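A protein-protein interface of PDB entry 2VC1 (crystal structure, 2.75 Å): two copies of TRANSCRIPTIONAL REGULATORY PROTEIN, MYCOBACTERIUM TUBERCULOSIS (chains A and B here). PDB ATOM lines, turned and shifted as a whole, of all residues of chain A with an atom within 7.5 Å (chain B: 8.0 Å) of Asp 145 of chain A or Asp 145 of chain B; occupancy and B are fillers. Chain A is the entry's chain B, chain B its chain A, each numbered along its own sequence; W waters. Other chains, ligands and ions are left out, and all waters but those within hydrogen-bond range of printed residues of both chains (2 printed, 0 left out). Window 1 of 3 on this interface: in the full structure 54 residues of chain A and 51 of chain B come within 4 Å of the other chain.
Ala 17 of chain A touches Ser 55 of chain B, and with the chains exchanged Ser 55 of chain A touches Ala 17 of chain B.
Glu 95 of chain A touches Ser 144 of chain B, and with the chains exchanged Ser 144 of chain A touches Glu 95 of chain B.
Tyr 98 of chain A touches Ser 144 of chain B, but with the chains exchanged Ser 144 of chain A does not touch Tyr 98 of chain B (4.3 Å).
Of the 31 pairs that touch across the chains among the printed residues, 26 have their exchanged pair printed and touching as well.
Of the 19 printed residues of chain B, 16 touch a printed residue of chain A.
Hydrophobic or aromatic side chains of chain A within 4 Å of the printed part of chain B: Val 94, Tyr 98 and Tyr 143.
Along chain A the printed residues that touch a printed residue of chain B span positions 17 to 147.
Among the printed residues, 31 pairs touch across the chains.
O of Ser 96 of chain B sits at hydrogen-bond distance from N of Leu 109 of chain B (3.1 Å).
The side-chain hydroxyl (OG) of Ser 144 of chain A lies within hydrogen-bond range of the side-chain carboxylate (OD2) of Asp 145 of chain A (2.8 Å).
The backbone carbonyl oxygen (O) of Ser 96 of chain A sits at hydrogen-bond distance from the backbone NH (N) of Leu 109 of chain A (3.2 Å).
The guanidinium group (NE) of Arg 111 of chain A is in salt-bridge range of the side-chain carboxylate (OE2) of Glu 95 of chain A (2.9 Å).
Ala 17 of chain B touches Ser 55 of chain A (O to CB, 3.3 Å).
Ser 55 of chain A touches Gln 147 of chain B (CB to NE2, 3.9 Å).
O of Cys 97 of chain A touches C of Thr 141 of chain B, 3.7 Å away.
CB of Ser 144 of chain B touches OH of Tyr 98 of chain A, at 3.9 Å.
Val 94 of chain B touches Tyr 143 of chain A.
Glu 95 of chain B touches Ser 144 of chain A.
Ser 144 of chain A touches Ser 96 of chain B (CA to OG, 3.8 Å).
OE1 of Gln 147 of chain A touches C of Arg 57 of chain B, 3.9 Å away.
Water W1 bridges OE2 of Glu 95 of chain A and N of His 148 of chain B.
Water W2 bridges OH of Tyr 98 of chain A (2.6 Å) and NH2 of Arg 111 of chain B (2.9 Å).
O of Glu 95 of chain B is in hydrogen-bond range of N of Asp 145 of chain A (3.1 Å).
The backbone NH (N) of Cys 97 of chain A is in hydrogen-bond range of the backbone carbonyl oxygen (O) of Tyr 143 of chain B.
The backbone NH (N) of Asp 145 of chain B is in hydrogen-bond range of the side-chain hydroxyl (OG) of Ser 96 of chain A, 3.3 Å away.
O of Arg 57 of chain A sits at hydrogen-bond distance from N of Gln 52 of chain B, at 2.8 Å.
N of Ser 55 of chain A lies within hydrogen-bond range of O of Ser 55 of chain B (2.9 Å).
O of Glu 95 of chain B lies within hydrogen-bond range of N of Arg 146 of chain A (3.0 Å).
The backbone carbonyl oxygen of Tyr 143 of chain A is in hydrogen-bond range of the backbone NH of Cys 97 of chain B (3.1 Å).
The backbone NH of Arg 146 of chain B is in hydrogen-bond range of the backbone carbonyl oxygen of Glu 95 of chain A (3.1 Å).
The backbone NH (N) of Asp 145 of chain A sits at hydrogen-bond distance from the side-chain hydroxyl (OG) of Ser 96 of chain B.
The backbone carbonyl oxygen (O) of Val 94 of chain B lies within hydrogen-bond range of the guanidinium group (NH1) of Arg 146 of chain A (2.9 Å).
O of Val 94 of chain A lies within hydrogen-bond range of NH1 of Arg 146 of chain B, at 2.5 Å.
OD1 of Asp 145 of chain B sits close to OD1 of Asp 145 of chain A, 3.4 Å away.
The backbone NH (N) of Asp 145 of chain B lies within hydrogen-bond range of the backbone carbonyl oxygen (O) of Glu 95 of chain A (3.5 Å).
O of Ala 56 of chain B lies within hydrogen-bond range of NE2 of Gln 147 of chain A, at 3.1 Å.
Printed residues of chain A within 4 Å of Ala 56 of chain B: Gln 147.
Of the printed residues of chain A, Arg 57 of chain B touches Gln 147 (3.9 Å).
Of chain A, only Glu 95 (3.5 Å), Ser 96 (3.3 Å) and Asp 145 (3.4 Å) come within 4 Å of Asp 145 of chain B.
The nearest residue of chain B that does not touch Asp 145 of chain A is Tyr 98 of chain B (5.7 Å).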
ATOM      1  N   ALA A  17       0.711   4.176   2.616  1.00  0.00           N
ATOM      2  CA  ALA A  17      -0.666   3.864   3.031  1.00  0.00           C
ATOM      3  C   ALA A  17      -1.212   4.972   3.872  1.00  0.00           C
ATOM      4  O   ALA A  17      -2.326   5.413   3.629  1.00  0.00           O
ATOM      5  CB  ALA A  17      -0.762   2.545   3.757  1.00  0.00           C
ATOM      6  N   SER A  55      -5.308   7.624  -3.968  1.00  0.00           N
ATOM      7  CA  SER A  55      -6.623   8.329  -3.970  1.00  0.00           C
ATOM      8  C   SER A  55      -6.674   9.348  -2.839  1.00  0.00           C
ATOM      9  O   SER A  55      -5.938   9.236  -1.902  1.00  0.00           O
ATOM     10  CB  SER A  55      -7.858   7.370  -3.988  1.00  0.00           C
ATOM     11  N   ARG A  57      -9.128  10.732  -0.130  1.00  0.00           N
ATOM     12  CA  ARG A  57     -10.291  10.232   0.548  1.00  0.00           C
ATOM     13  C   ARG A  57     -11.258  11.329   0.678  1.00  0.00           C
ATOM     14  O   ARG A  57     -11.092  12.222   1.484  1.00  0.00           O
ATOM     15  CB  ARG A  57      -9.892   9.723   1.901  1.00  0.00           C
ATOM     16  CG  ARG A  57      -9.657   8.167   1.856  1.00  0.00           C
ATOM     17  CD  ARG A  57      -8.461   7.836   2.748  1.00  0.00           C
ATOM     18  NE  ARG A  57      -8.642   8.476   4.075  1.00  0.00           N
ATOM     19  CZ  ARG A  57      -7.684   9.022   4.850  1.00  0.00           C
ATOM     20  NH1 ARG A  57      -6.384   9.016   4.483  1.00  0.00           N
ATOM     21  NH2 ARG A  57      -8.030   9.574   6.029  1.00  0.00           N
ATOM     22  N   VAL A  94     -22.869   2.723  -7.023  1.00  0.00           N
ATOM     23  CA  VAL A  94     -22.291   1.603  -6.318  1.00  0.00           C
ATOM     24  C   VAL A  94     -20.794   1.739  -6.203  1.00  0.00           C
ATOM     25  O   VAL A  94     -20.100   1.710  -7.138  1.00  0.00           O
ATOM     26  CB  VAL A  94     -22.860   0.175  -6.641  1.00  0.00           C
ATOM     27  CG1 VAL A  94     -23.987   0.181  -7.679  1.00  0.00           C
ATOM     28  CG2 VAL A  94     -21.794  -0.870  -6.787  1.00  0.00           C
ATOM     29  N   GLU A  95     -20.302   1.953  -5.018  1.00  0.00           N
ATOM     30  CA  GLU A  95     -18.925   2.110  -4.779  1.00  0.00           C
ATOM     31  C   GLU A  95     -18.159   0.783  -4.632  1.00  0.00           C
ATOM     32  O   GLU A  95     -16.983   0.792  -4.843  1.00  0.00           O
ATOM     33  CB  GLU A  95     -18.809   2.921  -3.496  1.00  0.00           C
ATOM     34  CG  GLU A  95     -17.436   3.322  -3.094  1.00  0.00           C
ATOM     35  CD  GLU A  95     -17.403   4.324  -1.905  1.00  0.00           C
ATOM     36  OE1 GLU A  95     -16.626   4.018  -0.955  1.00  0.00           O
ATOM     37  OE2 GLU A  95     -18.131   5.389  -1.915  1.00  0.00           O
ATOM     38  N   SER A  96     -18.738  -0.314  -4.142  1.00  0.00           N
ATOM     39  CA  SER A  96     -17.947  -1.504  -3.882  1.00  0.00           C
ATOM     40  C   SER A  96     -18.841  -2.674  -4.116  1.00  0.00           C
ATOM     41  O   SER A  96     -20.020  -2.559  -3.881  1.00  0.00           O
ATOM     42  CB  SER A  96     -17.532  -1.554  -2.456  1.00  0.00           C
ATOM     43  OG  SER A  96     -16.567  -0.573  -2.193  1.00  0.00           O
ATOM     44  N   CYS A  97     -18.307  -3.809  -4.560  1.00  0.00           N
ATOM     45  CA  CYS A  97     -19.129  -4.977  -4.731  1.00  0.00           C
ATOM     46  C   CYS A  97     -18.343  -6.265  -4.393  1.00  0.00           C
ATOM     47  O   CYS A  97     -17.249  -6.506  -4.920  1.00  0.00           O
ATOM     48  CB  CYS A  97     -19.625  -4.977  -6.117  1.00  0.00           C
ATOM     49  SG  CYS A  97     -20.342  -6.493  -6.565  1.00  0.00           S
ATOM     50  N   TYR A  98     -18.854  -7.050  -3.457  1.00  0.00           N
ATOM     51  CA  TYR A  98     -18.132  -8.237  -2.955  1.00  0.00           C
ATOM     52  C   TYR A  98     -18.991  -9.470  -3.134  1.00  0.00           C
ATOM     53  O   TYR A  98     -20.233  -9.384  -2.933  1.00  0.00           O
ATOM     54  CB  TYR A  98     -17.888  -8.113  -1.467  1.00  0.00           C
ATOM     55  CG  TYR A  98     -17.221  -6.845  -1.022  1.00  0.00           C
ATOM     56  CD1 TYR A  98     -17.962  -5.690  -0.584  1.00  0.00           C
ATOM     57  CD2 TYR A  98     -15.820  -6.799  -1.009  1.00  0.00           C
ATOM     58  CE1 TYR A  98     -17.274  -4.485  -0.187  1.00  0.00           C
ATOM     59  CE2 TYR A  98     -15.132  -5.641  -0.646  1.00  0.00           C
ATOM     60  CZ  TYR A  98     -15.837  -4.512  -0.242  1.00  0.00           C
ATOM     61  OH  TYR A  98     -15.001  -3.492   0.100  1.00  0.00           O
ATOM     62  N   LEU A 109     -21.594  -1.555  -1.306  1.00  0.00           N
ATOM     63  CA  LEU A 109     -21.706  -0.322  -0.524  1.00  0.00           C
ATOM     64  C   LEU A 109     -22.150   0.711  -1.535  1.00  0.00           C
ATOM     65  O   LEU A 109     -21.692   0.743  -2.674  1.00  0.00           O
ATOM     66  CB  LEU A 109     -20.381   0.030   0.090  1.00  0.00           C
ATOM     67  CG  LEU A 109     -20.376   1.413   0.713  1.00  0.00           C
ATOM     68  CD1 LEU A 109     -21.371   1.515   1.792  1.00  0.00           C
ATOM     69  CD2 LEU A 109     -19.100   1.489   1.345  1.00  0.00           C
ATOM     70  N   ARG A 111     -23.822   4.824  -2.130  1.00  0.00           N
ATOM     71  CA  ARG A 111     -24.105   6.171  -1.478  1.00  0.00           C
ATOM     72  C   ARG A 111     -25.061   6.966  -2.278  1.00  0.00           C
ATOM     73  O   ARG A 111     -25.086   6.840  -3.482  1.00  0.00           O
ATOM     74  CB  ARG A 111     -22.905   7.027  -1.289  1.00  0.00           C
ATOM     75  CG  ARG A 111     -21.695   6.277  -1.065  1.00  0.00           C
ATOM     76  CD  ARG A 111     -21.052   6.769   0.146  1.00  0.00           C
ATOM     77  NE  ARG A 111     -19.793   6.106   0.291  1.00  0.00           N
ATOM     78  CZ  ARG A 111     -19.250   5.820   1.470  1.00  0.00           C
ATOM     79  NH1 ARG A 111     -19.837   6.194   2.637  1.00  0.00           N
ATOM     80  NH2 ARG A 111     -18.099   5.177   1.479  1.00  0.00           N
ATOM     81  N   THR A 141     -19.756   6.610  10.043  1.00  0.00           N
ATOM     82  CA  THR A 141     -18.500   5.978   9.752  1.00  0.00           C
ATOM     83  C   THR A 141     -17.463   6.396  10.786  1.00  0.00           C
ATOM     84  O   THR A 141     -17.168   7.525  10.809  1.00  0.00           O
ATOM     85  CB  THR A 141     -18.074   6.390   8.365  1.00  0.00           C
ATOM     86  OG1 THR A 141     -19.057   5.895   7.464  1.00  0.00           O
ATOM     87  CG2 THR A 141     -16.830   5.717   7.975  1.00  0.00           C
ATOM     88  N   TYR A 143     -14.357   5.155  11.201  1.00  0.00           N
ATOM     89  CA  TYR A 143     -13.105   5.106  10.496  1.00  0.00           C
ATOM     90  C   TYR A 143     -13.251   4.118   9.396  1.00  0.00           C
ATOM     91  O   TYR A 143     -13.972   3.139   9.506  1.00  0.00           O
ATOM     92  CB  TYR A 143     -11.902   4.783  11.355  1.00  0.00           C
ATOM     93  CG  TYR A 143     -12.095   3.785  12.453  1.00  0.00           C
ATOM     94  CD1 TYR A 143     -12.558   4.188  13.729  1.00  0.00           C
ATOM     95  CD2 TYR A 143     -11.740   2.430  12.279  1.00  0.00           C
ATOM     96  CE1 TYR A 143     -12.690   3.244  14.811  1.00  0.00           C
ATOM     97  CE2 TYR A 143     -11.885   1.463  13.353  1.00  0.00           C
ATOM     98  CZ  TYR A 143     -12.351   1.887  14.587  1.00  0.00           C
ATOM     99  OH  TYR A 143     -12.489   0.988  15.608  1.00  0.00           O
ATOM    100  N   SER A 144     -12.549   4.392   8.334  1.00  0.00           N
ATOM    101  CA  SER A 144     -12.785   3.771   7.124  1.00  0.00           C
ATOM    102  C   SER A 144     -11.362   3.564   6.555  1.00  0.00           C
ATOM    103  O   SER A 144     -10.429   4.363   6.773  1.00  0.00           O
ATOM    104  CB  SER A 144     -13.587   4.783   6.346  1.00  0.00           C
ATOM    105  OG  SER A 144     -13.658   4.457   4.983  1.00  0.00           O
ATOM    106  N   ASP A 145     -11.170   2.437   5.886  1.00  0.00           N
ATOM    107  CA  ASP A 145      -9.900   2.124   5.228  1.00  0.00           C
ATOM    108  C   ASP A 145      -8.604   2.311   5.995  1.00  0.00           C
ATOM    109  O   ASP A 145      -7.678   2.770   5.367  1.00  0.00           O
ATOM    110  CB  ASP A 145      -9.712   3.006   3.993  1.00  0.00           C
ATOM    111  CG  ASP A 145     -11.006   3.311   3.297  1.00  0.00           C
ATOM    112  OD1 ASP A 145     -11.626   2.360   2.707  1.00  0.00           O
ATOM    113  OD2 ASP A 145     -11.387   4.518   3.341  1.00  0.00           O
ATOM    114  N   ARG A 146      -8.495   2.015   7.293  1.00  0.00           N
ATOM    115  CA  ARG A 146      -7.185   2.079   7.887  1.00  0.00           C
ATOM    116  C   ARG A 146      -6.513   0.782   7.530  1.00  0.00           C
ATOM    117  O   ARG A 146      -6.685  -0.171   8.268  1.00  0.00           O
ATOM    118  CB  ARG A 146      -7.163   2.190   9.406  1.00  0.00           C
ATOM    119  CG  ARG A 146      -8.373   2.530  10.133  1.00  0.00           C
ATOM    120  CD  ARG A 146      -7.923   2.803  11.548  1.00  0.00           C
ATOM    121  NE  ARG A 146      -8.334   1.938  12.672  1.00  0.00           N
ATOM    122  CZ  ARG A 146      -7.892   0.717  12.910  1.00  0.00           C
ATOM    123  NH1 ARG A 146      -7.090   0.091  12.065  1.00  0.00           N
ATOM    124  NH2 ARG A 146      -8.271   0.072  13.971  1.00  0.00           N
ATOM    125  N   GLN A 147      -5.782   0.751   6.399  1.00  0.00           N
ATOM    126  CA  GLN A 147      -4.848  -0.315   5.921  1.00  0.00           C
ATOM    127  C   GLN A 147      -3.735  -0.644   6.900  1.00  0.00           C
ATOM    128  O   GLN A 147      -3.083   0.222   7.420  1.00  0.00           O
ATOM    129  CB  GLN A 147      -4.208   0.058   4.578  1.00  0.00           C
ATOM    130  CG  GLN A 147      -5.212   0.024   3.445  1.00  0.00           C
ATOM    131  CD  GLN A 147      -4.831   0.767   2.176  1.00  0.00           C
ATOM    132  OE1 GLN A 147      -4.815   0.183   1.089  1.00  0.00           O
ATOM    133  NE2 GLN A 147      -4.569   2.056   2.294  1.00  0.00           N
ATOM    134  N   HIS A 148      -3.560  -1.925   7.151  1.00  0.00           N
ATOM    135  CA  HIS A 148      -2.629  -2.455   8.101  1.00  0.00           C
ATOM    136  C   HIS A 148      -1.637  -3.308   7.299  1.00  0.00           C
ATOM    137  O   HIS A 148      -2.089  -4.193   6.527  1.00  0.00           O
ATOM    138  CB  HIS A 148      -3.386  -3.373   9.036  1.00  0.00           C
ATOM    139  CG  HIS A 148      -2.494  -4.134   9.947  1.00  0.00           C
ATOM    140  ND1 HIS A 148      -1.455  -3.526  10.638  1.00  0.00           N
ATOM    141  CD2 HIS A 148      -2.457  -5.452  10.265  1.00  0.00           C
ATOM    142  CE1 HIS A 148      -0.805  -4.444  11.337  1.00  0.00           C
ATOM    143  NE2 HIS A 148      -1.400  -5.617  11.142  1.00  0.00           N
ATOM    144  N   ALA B  17      -9.581  12.242  -6.555  1.00  0.00           N
ATOM    145  CA  ALA B  17     -10.103  10.873  -6.271  1.00  0.00           C
ATOM    146  C   ALA B  17      -9.417   9.882  -7.193  1.00  0.00           C
ATOM    147  O   ALA B  17      -8.878   8.846  -6.757  1.00  0.00           O
ATOM    148  CB  ALA B  17     -11.638  10.808  -6.427  1.00  0.00           C
ATOM    149  N   GLN B  52      -9.872  14.005   3.314  1.00  0.00           N
ATOM    150  CA  GLN B  52      -9.640  13.505   4.688  1.00  0.00           C
ATOM    151  C   GLN B  52      -8.241  13.048   4.811  1.00  0.00           C
ATOM    152  O   GLN B  52      -7.711  12.969   5.915  1.00  0.00           O
ATOM    153  CB  GLN B  52     -10.575  12.387   5.065  1.00  0.00           C
ATOM    154  CG  GLN B  52     -11.907  12.616   4.472  1.00  0.00           C
ATOM    155  CD  GLN B  52     -12.960  11.913   5.231  1.00  0.00           C
ATOM    156  OE1 GLN B  52     -13.242  12.336   6.326  1.00  0.00           O
ATOM    157  NE2 GLN B  52     -13.563  10.855   4.674  1.00  0.00           N
ATOM    158  N   SER B  55      -4.142   8.245   0.324  1.00  0.00           N
ATOM    159  CA  SER B  55      -3.688   6.889   0.608  1.00  0.00           C
ATOM    160  C   SER B  55      -3.314   6.161  -0.673  1.00  0.00           C
ATOM    161  O   SER B  55      -4.024   6.302  -1.705  1.00  0.00           O
ATOM    162  CB  SER B  55      -4.754   6.125   1.347  1.00  0.00           C
ATOM    163  N   ALA B  56      -2.196   5.403  -0.655  1.00  0.00           N
ATOM    164  CA  ALA B  56      -1.945   4.342  -1.700  1.00  0.00           C
ATOM    165  C   ALA B  56      -2.992   3.217  -1.536  1.00  0.00           C
ATOM    166  O   ALA B  56      -3.287   2.862  -0.387  1.00  0.00           O
ATOM    167  CB  ALA B  56      -0.550   3.804  -1.546  1.00  0.00           C
ATOM    168  N   ARG B  57      -3.624   2.732  -2.625  1.00  0.00           N
ATOM    169  CA  ARG B  57      -4.509   1.541  -2.524  1.00  0.00           C
ATOM    170  C   ARG B  57      -3.579   0.321  -2.566  1.00  0.00           C
ATOM    171  O   ARG B  57      -2.932   0.073  -3.591  1.00  0.00           O
ATOM    172  CB  ARG B  57      -5.526   1.459  -3.640  1.00  0.00           C
ATOM    173  N   VAL B  94      -8.748  -4.330  12.289  1.00  0.00           N
ATOM    174  CA  VAL B  94      -9.981  -3.768  11.842  1.00  0.00           C
ATOM    175  C   VAL B  94      -9.822  -2.549  10.953  1.00  0.00           C
ATOM    176  O   VAL B  94      -9.303  -1.553  11.341  1.00  0.00           O
ATOM    177  CB  VAL B  94     -11.011  -3.690  12.952  1.00  0.00           C
ATOM    178  CG1 VAL B  94     -10.394  -4.027  14.241  1.00  0.00           C
ATOM    179  CG2 VAL B  94     -11.835  -2.447  12.878  1.00  0.00           C
ATOM    180  N   GLU B  95     -10.215  -2.664   9.710  1.00  0.00           N
ATOM    181  CA  GLU B  95     -10.001  -1.616   8.771  1.00  0.00           C
ATOM    182  C   GLU B  95     -11.121  -0.583   8.761  1.00  0.00           C
ATOM    183  O   GLU B  95     -10.882   0.546   8.381  1.00  0.00           O
ATOM    184  CB  GLU B  95      -9.951  -2.278   7.427  1.00  0.00           C
ATOM    185  CG  GLU B  95      -9.723  -1.360   6.234  1.00  0.00           C
ATOM    186  CD  GLU B  95      -9.262  -2.155   5.017  1.00  0.00           C
ATOM    187  OE1 GLU B  95      -9.925  -1.939   3.964  1.00  0.00           O
ATOM    188  OE2 GLU B  95      -8.270  -2.976   5.148  1.00  0.00           O
ATOM    189  N   SER B  96     -12.351  -0.952   9.139  1.00  0.00           N
ATOM    190  CA  SER B  96     -13.520  -0.018   9.106  1.00  0.00           C
ATOM    191  C   SER B  96     -14.489  -0.391  10.138  1.00  0.00           C
ATOM    192  O   SER B  96     -14.573  -1.544  10.505  1.00  0.00           O
ATOM    193  CB  SER B  96     -14.295  -0.186   7.828  1.00  0.00           C
ATOM    194  OG  SER B  96     -13.471   0.037   6.738  1.00  0.00           O
ATOM    195  N   CYS B  97     -15.289   0.578  10.528  1.00  0.00           N
ATOM    196  CA  CYS B  97     -16.203   0.472  11.636  1.00  0.00           C
ATOM    197  C   CYS B  97     -17.307   1.508  11.380  1.00  0.00           C
ATOM    198  O   CYS B  97     -17.078   2.754  11.322  1.00  0.00           O
ATOM    199  CB  CYS B  97     -15.497   0.658  12.960  1.00  0.00           C
ATOM    200  SG  CYS B  97     -16.716   0.680  14.341  1.00  0.00           S
ATOM    201  N   TYR B  98     -18.498   0.971  11.113  1.00  0.00           N
ATOM    202  CA  TYR B  98     -19.675   1.740  10.883  1.00  0.00           C
ATOM    203  C   TYR B  98     -20.771   1.400  11.871  1.00  0.00           C
ATOM    204  O   TYR B  98     -20.956   0.256  12.266  1.00  0.00           O
ATOM    205  CB  TYR B  98     -20.230   1.338   9.574  1.00  0.00           C
ATOM    206  CG  TYR B  98     -19.294   1.355   8.424  1.00  0.00           C
ATOM    207  CD1 TYR B  98     -18.643   0.207   8.035  1.00  0.00           C
ATOM    208  CD2 TYR B  98     -19.136   2.521   7.638  1.00  0.00           C
ATOM    209  CE1 TYR B  98     -17.769   0.206   6.912  1.00  0.00           C
ATOM    210  CE2 TYR B  98     -18.283   2.533   6.540  1.00  0.00           C
ATOM    211  CZ  TYR B  98     -17.593   1.381   6.208  1.00  0.00           C
ATOM    212  OH  TYR B  98     -16.712   1.392   5.156  1.00  0.00           O
ATOM    213  N   LEU B 109     -15.143  -4.106   8.897  1.00  0.00           N
ATOM    214  CA  LEU B 109     -14.468  -4.863   7.874  1.00  0.00           C
ATOM    215  C   LEU B 109     -13.100  -5.157   8.447  1.00  0.00           C
ATOM    216  O   LEU B 109     -12.416  -4.275   8.922  1.00  0.00           O
ATOM    217  CB  LEU B 109     -14.372  -4.097   6.537  1.00  0.00           C
ATOM    218  CG  LEU B 109     -13.479  -4.787   5.528  1.00  0.00           C
ATOM    219  CD1 LEU B 109     -14.257  -5.770   4.850  1.00  0.00           C
ATOM    220  CD2 LEU B 109     -13.092  -3.790   4.533  1.00  0.00           C
ATOM    221  N   ARG B 111      -9.451  -7.802   8.168  1.00  0.00           N
ATOM    222  CA  ARG B 111      -8.574  -8.590   7.237  1.00  0.00           C
ATOM    223  C   ARG B 111      -7.490  -9.341   7.989  1.00  0.00           C
ATOM    224  O   ARG B 111      -6.878  -8.840   8.920  1.00  0.00           O
ATOM    225  CB  ARG B 111      -7.889  -7.748   6.131  1.00  0.00           C
ATOM    226  CG  ARG B 111      -8.706  -6.708   5.507  1.00  0.00           C
ATOM    227  CD  ARG B 111      -8.271  -6.489   4.150  1.00  0.00           C
ATOM    228  NE  ARG B 111      -8.971  -5.336   3.519  1.00  0.00           N
ATOM    229  CZ  ARG B 111      -9.878  -5.393   2.518  1.00  0.00           C
ATOM    230  NH1 ARG B 111     -10.260  -6.557   1.976  1.00  0.00           N
ATOM    231  NH2 ARG B 111     -10.418  -4.255   2.055  1.00  0.00           N
ATOM    232  N   THR B 141     -13.500  -9.622  -4.047  1.00  0.00           N
ATOM    233  CA  THR B 141     -13.836  -8.210  -4.268  1.00  0.00           C
ATOM    234  C   THR B 141     -13.885  -7.925  -5.773  1.00  0.00           C
ATOM    235  O   THR B 141     -12.895  -8.067  -6.366  1.00  0.00           O
ATOM    236  CB  THR B 141     -12.770  -7.323  -3.724  1.00  0.00           C
ATOM    237  OG1 THR B 141     -12.744  -7.499  -2.322  1.00  0.00           O
ATOM    238  CG2 THR B 141     -13.093  -5.878  -3.908  1.00  0.00           C
ATOM    239  N   TYR B 143     -14.670  -4.803  -7.212  1.00  0.00           N
ATOM    240  CA  TYR B 143     -14.202  -3.404  -7.335  1.00  0.00           C
ATOM    241  C   TYR B 143     -14.477  -2.784  -5.974  1.00  0.00           C
ATOM    242  O   TYR B 143     -15.446  -3.238  -5.277  1.00  0.00           O
ATOM    243  CB  TYR B 143     -14.916  -2.592  -8.430  1.00  0.00           C
ATOM    244  CG  TYR B 143     -16.373  -2.907  -8.773  1.00  0.00           C
ATOM    245  CD1 TYR B 143     -16.698  -3.937  -9.712  1.00  0.00           C
ATOM    246  CD2 TYR B 143     -17.463  -2.146  -8.221  1.00  0.00           C
ATOM    247  CE1 TYR B 143     -18.069  -4.211 -10.078  1.00  0.00           C
ATOM    248  CE2 TYR B 143     -18.862  -2.403  -8.616  1.00  0.00           C
ATOM    249  CZ  TYR B 143     -19.145  -3.463  -9.525  1.00  0.00           C
ATOM    250  OH  TYR B 143     -20.460  -3.816  -9.891  1.00  0.00           O
ATOM    251  N   SER B 144     -13.682  -1.795  -5.556  1.00  0.00           N
ATOM    252  CA  SER B 144     -14.021  -1.112  -4.311  1.00  0.00           C
ATOM    253  C   SER B 144     -13.573   0.328  -4.310  1.00  0.00           C
ATOM    254  O   SER B 144     -12.928   0.753  -5.238  1.00  0.00           O
ATOM    255  CB  SER B 144     -13.464  -1.833  -3.101  1.00  0.00           C
ATOM    256  OG  SER B 144     -12.071  -2.032  -3.264  1.00  0.00           O
ATOM    257  N   ASP B 145     -13.909   1.087  -3.282  1.00  0.00           N
ATOM    258  CA  ASP B 145     -13.592   2.530  -3.278  1.00  0.00           C
ATOM    259  C   ASP B 145     -13.814   3.194  -4.606  1.00  0.00           C
ATOM    260  O   ASP B 145     -12.994   3.900  -5.054  1.00  0.00           O
ATOM    261  CB  ASP B 145     -12.126   2.825  -2.897  1.00  0.00           C
ATOM    262  CG  ASP B 145     -11.792   2.342  -1.527  1.00  0.00           C
ATOM    263  OD1 ASP B 145     -11.931   3.165  -0.564  1.00  0.00           O
ATOM    264  OD2 ASP B 145     -11.443   1.109  -1.422  1.00  0.00           O
ATOM    265  N   ARG B 146     -14.891   2.995  -5.296  1.00  0.00           N
ATOM    266  CA  ARG B 146     -14.909   3.765  -6.438  1.00  0.00           C
ATOM    267  C   ARG B 146     -15.713   5.034  -6.193  1.00  0.00           C
ATOM    268  O   ARG B 146     -16.903   5.017  -6.284  1.00  0.00           O
ATOM    269  CB  ARG B 146     -15.159   2.848  -7.621  1.00  0.00           C
ATOM    270  CG  ARG B 146     -16.484   2.656  -8.165  1.00  0.00           C
ATOM    271  CD  ARG B 146     -16.388   1.294  -8.631  1.00  0.00           C
ATOM    272  NE  ARG B 146     -17.030   1.034  -9.912  1.00  0.00           N
ATOM    273  CZ  ARG B 146     -18.317   1.086 -10.259  1.00  0.00           C
ATOM    274  NH1 ARG B 146     -19.304   1.494  -9.482  1.00  0.00           N
ATOM    275  NH2 ARG B 146     -18.599   0.730 -11.509  1.00  0.00           N
ATOM    276  N   GLN B 147     -15.037   6.120  -5.772  1.00  0.00           N
ATOM    277  CA  GLN B 147     -15.701   7.335  -5.205  1.00  0.00           C
ATOM    278  C   GLN B 147     -16.372   8.089  -6.295  1.00  0.00           C
ATOM    279  O   GLN B 147     -15.745   8.307  -7.272  1.00  0.00           O
ATOM    280  CB  GLN B 147     -14.729   8.273  -4.474  1.00  0.00           C
ATOM    281  CG  GLN B 147     -13.738   7.523  -3.702  1.00  0.00           C
ATOM    282  CD  GLN B 147     -12.877   8.367  -2.866  1.00  0.00           C
ATOM    283  OE1 GLN B 147     -13.376   9.069  -1.994  1.00  0.00           O
ATOM    284  NE2 GLN B 147     -11.558   8.274  -3.069  1.00  0.00           N
ATOM    285  N   HIS B 148     -17.624   8.502  -6.124  1.00  0.00           N
ATOM    286  CA  HIS B 148     -18.417   9.171  -7.148  1.00  0.00           C
ATOM    287  C   HIS B 148     -18.600  10.629  -6.775  1.00  0.00           C
ATOM    288  O   HIS B 148     -19.162  10.946  -5.706  1.00  0.00           O
ATOM    289  CB  HIS B 148     -19.738   8.481  -7.175  1.00  0.00           C
ATOM    290  CG  HIS B 148     -20.763   9.144  -8.033  1.00  0.00           C
ATOM    291  ND1 HIS B 148     -20.481   9.620  -9.305  1.00  0.00           N
ATOM    292  CD2 HIS B 148     -22.094   9.335  -7.839  1.00  0.00           C
ATOM    293  CE1 HIS B 148     -21.590  10.120  -9.835  1.00  0.00           C
ATOM    294  NE2 HIS B 148     -22.579   9.963  -8.963  1.00  0.00           N
HETATM  295  O   HOH W   1     -19.134   6.914  -3.665  1.00  0.00           O
HETATM  296  O   HOH W   2     -12.429  -3.178   0.243  1.00  0.00           O
